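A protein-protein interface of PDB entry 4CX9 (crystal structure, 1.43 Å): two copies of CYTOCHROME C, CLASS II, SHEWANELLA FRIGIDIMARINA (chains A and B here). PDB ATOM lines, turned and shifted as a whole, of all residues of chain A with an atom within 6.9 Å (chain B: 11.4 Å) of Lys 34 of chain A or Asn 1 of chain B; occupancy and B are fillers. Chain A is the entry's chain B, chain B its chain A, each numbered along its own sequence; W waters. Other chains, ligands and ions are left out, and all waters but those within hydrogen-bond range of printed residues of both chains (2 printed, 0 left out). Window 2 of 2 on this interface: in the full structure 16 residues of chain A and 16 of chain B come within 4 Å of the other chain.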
ATOM      1  N   TYR A  21      14.299  16.105  28.590  1.00  0.00           N
ATOM      2  CA  TYR A  21      14.271  14.676  28.871  1.00  0.00           C
ATOM      3  C   TYR A  21      13.115  14.008  28.121  1.00  0.00           C
ATOM      4  O   TYR A  21      13.262  12.947  27.471  1.00  0.00           O
ATOM      5  CB  TYR A  21      14.091  14.458  30.372  1.00  0.00           C
ATOM      6  CG  TYR A  21      13.949  12.999  30.794  1.00  0.00           C
ATOM      7  CD1 TYR A  21      15.044  12.215  30.998  1.00  0.00           C
ATOM      8  CD2 TYR A  21      12.688  12.413  30.950  1.00  0.00           C
ATOM      9  CE1 TYR A  21      14.920  10.878  31.365  1.00  0.00           C
ATOM     10  CE2 TYR A  21      12.548  11.099  31.329  1.00  0.00           C
ATOM     11  CZ  TYR A  21      13.663  10.335  31.539  1.00  0.00           C
ATOM     12  OH  TYR A  21      13.551   8.986  31.912  1.00  0.00           O
ATOM     13  N   GLY A  24      13.623  14.326  24.296  1.00  0.00           N
ATOM     14  CA  GLY A  24      14.695  13.413  23.842  1.00  0.00           C
ATOM     15  C   GLY A  24      14.198  11.979  23.747  1.00  0.00           C
ATOM     16  O   GLY A  24      14.669  11.230  22.871  1.00  0.00           O
ATOM     17  N   ASP A  25      13.248  11.580  24.595  1.00  0.00           N
ATOM     18  CA  ASP A  25      12.690  10.208  24.473  1.00  0.00           C
ATOM     19  C   ASP A  25      11.891  10.037  23.171  1.00  0.00           C
ATOM     20  O   ASP A  25      11.981   9.002  22.461  1.00  0.00           O
ATOM     21  CB  ASP A  25      11.859   9.861  25.731  1.00  0.00           C
ATOM     22  CG  ASP A  25      11.634   8.347  25.881  1.00  0.00           C
ATOM     23  OD1 ASP A  25      12.633   7.602  25.680  1.00  0.00           O
ATOM     24  OD2 ASP A  25      10.489   7.913  26.146  1.00  0.00           O
ATOM     25  N   MET A  26      11.129  11.049  22.779  1.00  0.00           N
ATOM     26  CA  MET A  26      10.454  11.033  21.489  1.00  0.00           C
ATOM     27  C   MET A  26      11.502  10.965  20.367  1.00  0.00           C
ATOM     28  O   MET A  26      11.323  10.190  19.382  1.00  0.00           O
ATOM     29  CB  MET A  26       9.574  12.253  21.306  1.00  0.00           C
ATOM     30  CG  MET A  26       8.281  12.213  22.137  1.00  0.00           C
ATOM     31  SD  MET A  26       7.148  13.545  21.726  1.00  0.00           S
ATOM     32  CE  MET A  26       7.991  14.829  22.602  1.00  0.00           C
ATOM     33  N   GLY A  27      12.552  11.772  20.487  1.00  0.00           N
ATOM     34  CA  GLY A  27      13.632  11.748  19.459  1.00  0.00           C
ATOM     35  C   GLY A  27      14.237  10.339  19.343  1.00  0.00           C
ATOM     36  O   GLY A  27      14.464   9.836  18.233  1.00  0.00           O
ATOM     37  N   ALA A  28      14.503   9.717  20.476  1.00  0.00           N
ATOM     38  CA  ALA A  28      15.089   8.350  20.503  1.00  0.00           C
ATOM     39  C   ALA A  28      14.208   7.371  19.750  1.00  0.00           C
ATOM     40  O   ALA A  28      14.689   6.543  18.913  1.00  0.00           O
ATOM     41  CB  ALA A  28      15.328   7.890  21.912  1.00  0.00           C
ATOM     42  N   MET A  29      12.911   7.465  19.967  1.00  0.00           N
ATOM     43  CA  MET A  29      11.993   6.625  19.220  1.00  0.00           C
ATOM     44  C   MET A  29      11.981   6.917  17.731  1.00  0.00           C
ATOM     45  O   MET A  29      12.007   5.988  16.936  1.00  0.00           O
ATOM     46  CB  MET A  29      10.585   6.670  19.805  1.00  0.00           C
ATOM     47  CG  MET A  29      10.551   6.113  21.212  1.00  0.00           C
ATOM     48  SD  MET A  29       8.821   6.178  21.836  1.00  0.00           S
ATOM     49  CE  MET A  29       9.076   5.790  23.510  1.00  0.00           C
ATOM     50  N   LEU A  30      12.003   8.179  17.336  1.00  0.00           N
ATOM     51  CA  LEU A  30      11.923   8.491  15.907  1.00  0.00           C
ATOM     52  C   LEU A  30      13.248   8.264  15.181  1.00  0.00           C
ATOM     53  O   LEU A  30      13.233   8.047  13.973  1.00  0.00           O
ATOM     54  CB  LEU A  30      11.481   9.928  15.703  1.00  0.00           C
ATOM     55  CG  LEU A  30      10.054  10.161  16.180  1.00  0.00           C
ATOM     56  CD1 LEU A  30       9.811  11.652  16.151  1.00  0.00           C
ATOM     57  CD2 LEU A  30       8.997   9.430  15.349  1.00  0.00           C
ATOM     58  N   LYS A  31      14.357   8.306  15.892  1.00  0.00           N
ATOM     59  CA  LYS A  31      15.687   8.211  15.271  1.00  0.00           C
ATOM     60  C   LYS A  31      16.089   6.747  15.175  1.00  0.00           C
ATOM     61  O   LYS A  31      17.091   6.425  14.540  1.00  0.00           O
ATOM     62  CB  LYS A  31      16.726   9.020  16.071  1.00  0.00           C
ATOM     63  N   GLY A  32      15.310   5.861  15.813  1.00  0.00           N
ATOM     64  CA  GLY A  32      15.628   4.432  15.887  1.00  0.00           C
ATOM     65  C   GLY A  32      16.552   3.961  16.980  1.00  0.00           C
ATOM     66  O   GLY A  32      16.938   2.784  16.971  1.00  0.00           O
ATOM     67  N   LYS A  33      16.838   4.797  17.977  1.00  0.00           N
ATOM     68  CA  LYS A  33      17.633   4.359  19.135  1.00  0.00           C
ATOM     69  C   LYS A  33      16.832   3.343  19.950  1.00  0.00           C
ATOM     70  O   LYS A  33      17.383   2.429  20.540  1.00  0.00           O
ATOM     71  CB  LYS A  33      18.044   5.531  20.043  1.00  0.00           C
ATOM     72  CG  LYS A  33      18.741   5.096  21.330  1.00  0.00           C
ATOM     73  CD  LYS A  33      19.575   6.184  21.985  1.00  0.00           C
ATOM     74  CE  LYS A  33      19.906   5.743  23.401  1.00  0.00           C
ATOM     75  NZ  LYS A  33      20.962   6.533  24.069  1.00  0.00           N
ATOM     76  N   LYS A  34      15.504   3.511  19.967  1.00  0.00           N
ATOM     77  CA  LYS A  34      14.588   2.575  20.657  1.00  0.00           C
ATOM     78  C   LYS A  34      13.332   2.475  19.827  1.00  0.00           C
ATOM     79  O   LYS A  34      13.086   3.322  19.014  1.00  0.00           O
ATOM     80  CB  LYS A  34      14.300   3.023  22.109  1.00  0.00           C
ATOM     81  CG  LYS A  34      13.516   4.315  22.192  1.00  0.00           C
ATOM     82  CD  LYS A  34      13.703   5.013  23.525  1.00  0.00           C
ATOM     83  CE  LYS A  34      13.108   4.241  24.648  1.00  0.00           C
ATOM     84  NZ  LYS A  34      13.335   4.920  25.967  1.00  0.00           N
ATOM     85  N   PRO A  35      12.556   1.362  19.960  1.00  0.00           N
ATOM     86  CA  PRO A  35      11.403   1.149  19.081  1.00  0.00           C
ATOM     87  C   PRO A  35      10.334   2.160  19.441  1.00  0.00           C
ATOM     88  O   PRO A  35      10.239   2.568  20.597  1.00  0.00           O
ATOM     89  CB  PRO A  35      10.932  -0.298  19.388  1.00  0.00           C
ATOM     90  CG  PRO A  35      11.669  -0.694  20.621  1.00  0.00           C
ATOM     91  CD  PRO A  35      12.870   0.195  20.791  1.00  0.00           C
ATOM     92  N   PHE A  36       9.569   2.562  18.438  1.00  0.00           N
ATOM     93  CA  PHE A  36       8.481   3.470  18.607  1.00  0.00           C
ATOM     94  C   PHE A  36       7.403   2.741  19.424  1.00  0.00           C
ATOM     95  O   PHE A  36       7.032   1.617  19.086  1.00  0.00           O
ATOM     96  CB  PHE A  36       7.937   3.937  17.280  1.00  0.00           C
ATOM     97  CG  PHE A  36       6.821   4.897  17.421  1.00  0.00           C
ATOM     98  CD1 PHE A  36       5.544   4.425  17.517  1.00  0.00           C
ATOM     99  CD2 PHE A  36       7.050   6.274  17.483  1.00  0.00           C
ATOM    100  CE1 PHE A  36       4.477   5.287  17.675  1.00  0.00           C
ATOM    101  CE2 PHE A  36       5.991   7.124  17.654  1.00  0.00           C
ATOM    102  CZ  PHE A  36       4.706   6.652  17.706  1.00  0.00           C
ATOM    103  N   ASP A  37       6.967   3.373  20.521  1.00  0.00           N
ATOM    104  CA  ASP A  37       5.913   2.837  21.417  1.00  0.00           C
ATOM    105  C   ASP A  37       4.860   3.932  21.505  1.00  0.00           C
ATOM    106  O   ASP A  37       5.166   5.007  22.149  1.00  0.00           O
ATOM    107  CB  ASP A  37       6.533   2.589  22.799  1.00  0.00           C
ATOM    108  CG  ASP A  37       5.534   2.080  23.846  1.00  0.00           C
ATOM    109  OD1 ASP A  37       4.394   2.542  23.905  1.00  0.00           O
ATOM    110  OD2 ASP A  37       5.850   1.145  24.579  1.00  0.00           O
ATOM    111  N   VAL A  40       3.861   5.332  25.156  1.00  0.00           N
ATOM    112  CA  VAL A  40       4.865   6.148  25.807  1.00  0.00           C
ATOM    113  C   VAL A  40       5.052   7.472  25.025  1.00  0.00           C
ATOM    114  O   VAL A  40       5.116   8.568  25.624  1.00  0.00           O
ATOM    115  CB  VAL A  40       6.188   5.365  25.995  1.00  0.00           C
ATOM    116  CG1 VAL A  40       7.264   6.241  26.577  1.00  0.00           C
ATOM    117  CG2 VAL A  40       5.958   4.154  26.900  1.00  0.00           C
ATOM    118  N   ARG A  44       4.922  11.272  26.432  1.00  0.00           N
ATOM    119  CA  ARG A  44       6.032  12.207  26.269  1.00  0.00           C
ATOM    120  C   ARG A  44       5.571  13.501  25.579  1.00  0.00           C
ATOM    121  O   ARG A  44       5.968  14.620  25.962  1.00  0.00           O
ATOM    122  CB  ARG A  44       7.181  11.610  25.450  1.00  0.00           C
ATOM    123  CG  ARG A  44       7.797  10.388  26.110  1.00  0.00           C
ATOM    124  CD  ARG A  44       8.397  10.735  27.470  1.00  0.00           C
ATOM    125  NE  ARG A  44       9.036   9.554  28.029  1.00  0.00           N
ATOM    126  CZ  ARG A  44       9.386   9.422  29.308  1.00  0.00           C
ATOM    127  NH1 ARG A  44       9.111  10.366  30.206  1.00  0.00           N
ATOM    128  NH2 ARG A  44       9.934   8.286  29.714  1.00  0.00           N
ATOM    129  N   ASN B   1      15.208   5.701  31.700  1.00  0.00           N
ATOM    130  CA  ASN B   1      15.994   6.566  30.734  1.00  0.00           C
ATOM    131  C   ASN B   1      17.115   7.389  31.378  1.00  0.00           C
ATOM    132  O   ASN B   1      17.813   8.120  30.691  1.00  0.00           O
ATOM    133  CB  ASN B   1      15.087   7.475  29.885  1.00  0.00           C
ATOM    134  CG  ASN B   1      15.349   7.362  28.366  1.00  0.00           C
ATOM    135  OD1 ASN B   1      15.655   6.292  27.868  1.00  0.00           O
ATOM    136  ND2 ASN B   1      15.139   8.450  27.626  1.00  0.00           N
ATOM    137  N   PHE B   2      17.307   7.277  32.691  1.00  0.00           N
ATOM    138  CA  PHE B   2      18.318   8.099  33.363  1.00  0.00           C
ATOM    139  C   PHE B   2      19.728   7.565  33.189  1.00  0.00           C
ATOM    140  O   PHE B   2      19.983   6.403  33.427  1.00  0.00           O
ATOM    141  CB  PHE B   2      17.966   8.235  34.808  1.00  0.00           C
ATOM    142  CG  PHE B   2      16.588   8.859  35.011  1.00  0.00           C
ATOM    143  CD1 PHE B   2      16.354  10.184  34.676  1.00  0.00           C
ATOM    144  CD2 PHE B   2      15.538   8.111  35.486  1.00  0.00           C
ATOM    145  CE1 PHE B   2      15.083  10.752  34.882  1.00  0.00           C
ATOM    146  CE2 PHE B   2      14.284   8.675  35.699  1.00  0.00           C
ATOM    147  CZ  PHE B   2      14.072   9.982  35.366  1.00  0.00           C
ATOM    148  N   GLU B   3      20.621   8.463  32.802  1.00  0.00           N
ATOM    149  CA  GLU B   3      22.025   8.107  32.592  1.00  0.00           C
ATOM    150  C   GLU B   3      22.652   7.631  33.910  1.00  0.00           C
ATOM    151  O   GLU B   3      23.285   6.584  33.962  1.00  0.00           O
ATOM    152  CB  GLU B   3      22.812   9.282  31.989  1.00  0.00           C
ATOM    153  CG  GLU B   3      22.223   9.929  30.730  1.00  0.00           C
ATOM    154  N   GLU B   4      22.477   8.414  34.976  1.00  0.00           N
ATOM    155  CA  GLU B   4      22.927   8.073  36.323  1.00  0.00           C
ATOM    156  C   GLU B   4      21.784   8.274  37.318  1.00  0.00           C
ATOM    157  O   GLU B   4      20.894   9.081  37.065  1.00  0.00           O
ATOM    158  CB  GLU B   4      24.092   9.023  36.724  1.00  0.00           C
ATOM    159  CG  GLU B   4      25.381   8.769  35.925  1.00  0.00           C
ATOM    160  N   PRO B   5      21.828   7.619  38.482  1.00  0.00           N
ATOM    161  CA  PRO B   5      20.788   7.855  39.499  1.00  0.00           C
ATOM    162  C   PRO B   5      20.637   9.293  39.923  1.00  0.00           C
ATOM    163  O   PRO B   5      19.519   9.726  40.250  1.00  0.00           O
ATOM    164  CB  PRO B   5      21.256   7.000  40.684  1.00  0.00           C
ATOM    165  CG  PRO B   5      21.971   5.897  40.006  1.00  0.00           C
ATOM    166  CD  PRO B   5      22.738   6.531  38.902  1.00  0.00           C
ATOM    167  N   ALA B   6      21.737  10.058  39.952  1.00  0.00           N
ATOM    168  CA  ALA B   6      21.623  11.436  40.334  1.00  0.00           C
ATOM    169  C   ALA B   6      20.651  12.154  39.373  1.00  0.00           C
ATOM    170  O   ALA B   6      19.998  13.117  39.779  1.00  0.00           O
ATOM    171  CB  ALA B   6      22.979  12.128  40.296  1.00  0.00           C
ATOM    172  N   ASP B   7      20.579  11.705  38.124  1.00  0.00           N
ATOM    173  CA  ASP B   7      19.707  12.375  37.153  1.00  0.00           C
ATOM    174  C   ASP B   7      18.230  12.120  37.506  1.00  0.00           C
ATOM    175  O   ASP B   7      17.390  12.998  37.329  1.00  0.00           O
ATOM    176  CB  ASP B   7      19.973  11.878  35.728  1.00  0.00           C
ATOM    177  CG  ASP B   7      21.397  12.178  35.227  1.00  0.00           C
ATOM    178  OD1 ASP B   7      21.984  13.158  35.656  1.00  0.00           O
ATOM    179  OD2 ASP B   7      21.897  11.401  34.411  1.00  0.00           O
ATOM    180  N   ALA B   8      17.946  10.929  37.993  1.00  0.00           N
ATOM    181  CA  ALA B   8      16.565  10.585  38.412  1.00  0.00           C
ATOM    182  C   ALA B   8      16.152  11.468  39.584  1.00  0.00           C
ATOM    183  O   ALA B   8      14.973  11.967  39.671  1.00  0.00           O
ATOM    184  CB  ALA B   8      16.508   9.114  38.806  1.00  0.00           C
ATOM    185  N   ILE B   9      17.073  11.669  40.549  1.00  0.00           N
ATOM    186  CA  ILE B   9      16.832  12.542  41.665  1.00  0.00           C
ATOM    187  C   ILE B   9      16.597  14.005  41.257  1.00  0.00           C
ATOM    188  O   ILE B   9      15.622  14.659  41.689  1.00  0.00           O
ATOM    189  CB  ILE B   9      18.005  12.467  42.687  1.00  0.00           C
ATOM    190  CG1 ILE B   9      17.993  11.098  43.335  1.00  0.00           C
ATOM    191  CG2 ILE B   9      17.847  13.512  43.753  1.00  0.00           C
ATOM    192  CD1 ILE B   9      19.331  10.725  44.026  1.00  0.00           C
ATOM    193  N   TYR B  11      15.649  15.080  38.437  1.00  0.00           N
ATOM    194  CA  TYR B  11      14.391  15.136  37.640  1.00  0.00           C
ATOM    195  C   TYR B  11      13.170  15.288  38.564  1.00  0.00           C
ATOM    196  O   TYR B  11      12.313  16.209  38.396  1.00  0.00           O
ATOM    197  CB  TYR B  11      14.309  13.899  36.777  1.00  0.00           C
ATOM    198  CG  TYR B  11      13.099  13.800  35.834  1.00  0.00           C
ATOM    199  CD1 TYR B  11      13.160  14.305  34.566  1.00  0.00           C
ATOM    200  CD2 TYR B  11      11.911  13.136  36.217  1.00  0.00           C
ATOM    201  CE1 TYR B  11      12.084  14.202  33.700  1.00  0.00           C
ATOM    202  CE2 TYR B  11      10.834  13.062  35.336  1.00  0.00           C
ATOM    203  CZ  TYR B  11      10.940  13.593  34.093  1.00  0.00           C
ATOM    204  OH  TYR B  11       9.894  13.510  33.172  1.00  0.00           O
ATOM    205  N   ILE B  54       4.601  13.961  36.398  1.00  0.00           N
ATOM    206  CA  ILE B  54       6.025  13.959  36.024  1.00  0.00           C
ATOM    207  C   ILE B  54       6.993  13.274  37.053  1.00  0.00           C
ATOM    208  O   ILE B  54       7.819  12.507  36.638  1.00  0.00           O
ATOM    209  CB  ILE B  54       6.518  15.392  35.738  1.00  0.00           C
ATOM    210  CG1 ILE B  54       5.670  16.048  34.647  1.00  0.00           C
ATOM    211  CG2 ILE B  54       8.022  15.380  35.380  1.00  0.00           C
ATOM    212  CD1 ILE B  54       5.821  15.455  33.319  1.00  0.00           C
ATOM    213  N   HIS B  56       6.970  10.955  39.399  1.00  0.00           N
ATOM    214  CA  HIS B  56       6.991   9.546  39.784  1.00  0.00           C
ATOM    215  C   HIS B  56       8.110   8.784  39.074  1.00  0.00           C
ATOM    216  O   HIS B  56       8.767   7.898  39.661  1.00  0.00           O
ATOM    217  CB  HIS B  56       5.625   8.900  39.523  1.00  0.00           C
ATOM    218  CG  HIS B  56       5.602   7.439  39.812  1.00  0.00           C
ATOM    219  ND1 HIS B  56       5.818   6.487  38.850  1.00  0.00           N
ATOM    220  CD2 HIS B  56       5.396   6.766  40.962  1.00  0.00           C
ATOM    221  CE1 HIS B  56       5.744   5.281  39.391  1.00  0.00           C
ATOM    222  NE2 HIS B  56       5.491   5.430  40.673  1.00  0.00           N
ATOM    223  N   GLU B  57       8.332   9.068  37.797  1.00  0.00           N
ATOM    224  CA  GLU B  57       9.309   8.382  36.986  1.00  0.00           C
ATOM    225  C   GLU B  57      10.726   8.404  37.612  1.00  0.00           C
ATOM    226  O   GLU B  57      11.525   7.497  37.380  1.00  0.00           O
ATOM    227  CB  GLU B  57       9.342   9.007  35.586  1.00  0.00           C
ATOM    228  CG  GLU B  57      10.312   8.328  34.616  1.00  0.00           C
ATOM    229  CD  GLU B  57      10.269   8.825  33.196  1.00  0.00           C
ATOM    230  OE1 GLU B  57       9.475   9.757  32.883  1.00  0.00           O
ATOM    231  OE2 GLU B  57      11.026   8.267  32.359  1.00  0.00           O
ATOM    232  N   GLY B  58      11.013   9.433  38.398  1.00  0.00           N
ATOM    233  CA  GLY B  58      12.308   9.563  39.029  1.00  0.00           C
ATOM    234  C   GLY B  58      12.579   8.664  40.210  1.00  0.00           C
ATOM    235  O   GLY B  58      13.749   8.589  40.648  1.00  0.00           O
ATOM    236  N   PHE B  59      11.573   7.993  40.748  1.00  0.00           N
ATOM    237  CA  PHE B  59      11.740   7.175  41.950  1.00  0.00           C
ATOM    238  C   PHE B  59      12.220   5.746  41.675  1.00  0.00           C
ATOM    239  O   PHE B  59      11.563   4.739  41.975  1.00  0.00           O
ATOM    240  CB  PHE B  59      10.482   7.231  42.794  1.00  0.00           C
ATOM    241  CG  PHE B  59      10.281   8.592  43.441  1.00  0.00           C
ATOM    242  CD1 PHE B  59      10.833   8.877  44.660  1.00  0.00           C
ATOM    243  CD2 PHE B  59       9.518   9.594  42.821  1.00  0.00           C
ATOM    244  CE1 PHE B  59      10.701  10.093  45.280  1.00  0.00           C
ATOM    245  CE2 PHE B  59       9.356  10.828  43.466  1.00  0.00           C
ATOM    246  CZ  PHE B  59       9.940  11.084  44.700  1.00  0.00           C
ATOM    247  N   ILE B  60      13.414   5.682  41.111  1.00  0.00           N
ATOM    248  CA  ILE B  60      14.034   4.429  40.693  1.00  0.00           C
ATOM    249  C   ILE B  60      14.711   3.731  41.883  1.00  0.00           C
ATOM    250  O   ILE B  60      15.087   4.358  42.880  1.00  0.00           O
ATOM    251  CB  ILE B  60      15.025   4.656  39.541  1.00  0.00           C
ATOM    252  CG1 ILE B  60      16.230   5.503  39.982  1.00  0.00           C
ATOM    253  CG2 ILE B  60      14.297   5.278  38.356  1.00  0.00           C
ATOM    254  CD1 ILE B  60      17.354   5.532  38.954  1.00  0.00           C
ATOM    255  N   ALA B  61      14.778   2.391  41.801  1.00  0.00           N
ATOM    256  CA  ALA B  61      15.394   1.633  42.882  1.00  0.00           C
ATOM    257  C   ALA B  61      16.825   2.146  43.172  1.00  0.00           C
ATOM    258  O   ALA B  61      17.549   2.508  42.263  1.00  0.00           O
ATOM    259  CB  ALA B  61      15.431   0.142  42.501  1.00  0.00           C
HETATM  260  O   HOH W   1      15.362  11.176  27.473  1.00  0.00           O
HETATM  261  O   HOH W   2      12.509   5.937  33.002  1.00  0.00           O
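OD1 of Asp 25 of chain A lies within hydrogen-bond range of ND2 of Asn 1 of chain B (3.3 Å). The side-chain amide oxygen (OD1) of Asn 1 of chain B sits at hydrogen-bond distance from the side-chain amino group (NZ) of Lys 34 of chain A (3.3 Å). OE2 of Glu 57 of chain B sits at hydrogen-bond distance from OH of Tyr 21 of chain A, at 2.7 Å. The guanidinium group (NH1) of Arg 44 of chain A is in salt-bridge range of the side-chain carboxylate (OE1) of Glu 57 of chain B (2.8 Å).
The side-chain carboxylate (OD1) of Asp 25 of chain A lies within salt-bridge range of the side-chain amino group (NZ) of Lys 34 of chain A (2.8 Å). OD2 of Asp 25 of chain A is in salt-bridge range of NE of Arg 44 of chain A (2.9 Å). The backbone NH (N) of Lys 34 of chain A lies within hydrogen-bond range of the backbone carbonyl oxygen (O) of Ala 28 of chain A.
OH of Tyr 21 of chain A touches CB of Asn 1 of chain B (3.0 Å). Tyr 21 of chain A touches Phe 2 of chain B (CE1 to CE1, 3.5 Å). Tyr 11 of chain B touches Tyr 21 of chain A.
No residue of chain B comes within 4 Å of Gly 24 of chain A. Printed residues of chain B within 4 Å of Asp 25 of chain A: Asn 1 (3.3 Å). No residue of chain B comes within 4 Å of Met 29 of chain A. No residue of chain B comes within 4 Å of Lys 31 of chain A. No residue of chain B comes within 4 Å of Lys 33 of chain A. Of the printed residues of chain B, Lys 34 of chain A touches Asn 1. Of the printed residues of chain A, Asn 1 of chain B touches Tyr 21 (3.0 Å), Asp 25 (3.3 Å) and Lys 34 (3.3 Å). Ile 9 of chain B touches none of the printed residues of chain A. Of the printed residues of chain A, Tyr 11 of chain B touches Tyr 21 (3.3 Å). Phe 59 of chain B touches none of the printed residues of chain A. The nearest printed residue of chain B that does not touch Lys 34 of chain A is Glu 57 of chain B (7.6 Å). The nearest printed residue of chain A that does not touch Asn 1 of chain B is Arg 44 of chain A (5.2 Å).
Printed residues of chain A that touch a printed residue of chain B: Tyr 21, Asp 25, Lys 34 and Arg 44. Hydrophobic or aromatic side chains of chain A within 4 Å of the printed part of chain B: Tyr 21. Printed residues of chain B that touch a printed residue of chain A: Asn 1, Phe 2, Tyr 11 and Glu 57. Hydrophobic or aromatic side chains of chain B that line the printed part of chain A: Phe 2 and Tyr 11. Among the printed residues, Asp or Glu carboxylates within 4 Å of a Lys or Arg side-chain nitrogen of the other chain: Arg 44 of chain A with Glu 57 of chain B (2.8 Å).
No position is printed for both chains.
Water W1 lies within hydrogen-bond range of the side-chain amide nitrogen of Asn 1 of chain B (2.7 Å) and the backbone carbonyl oxygen of Tyr 21 of chain A (2.7 Å). Water W2 lies within hydrogen-bond range of OE2 of Glu 57 of chain B, N of Asn 1 of chain B and OH of Tyr 21 of chain A.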
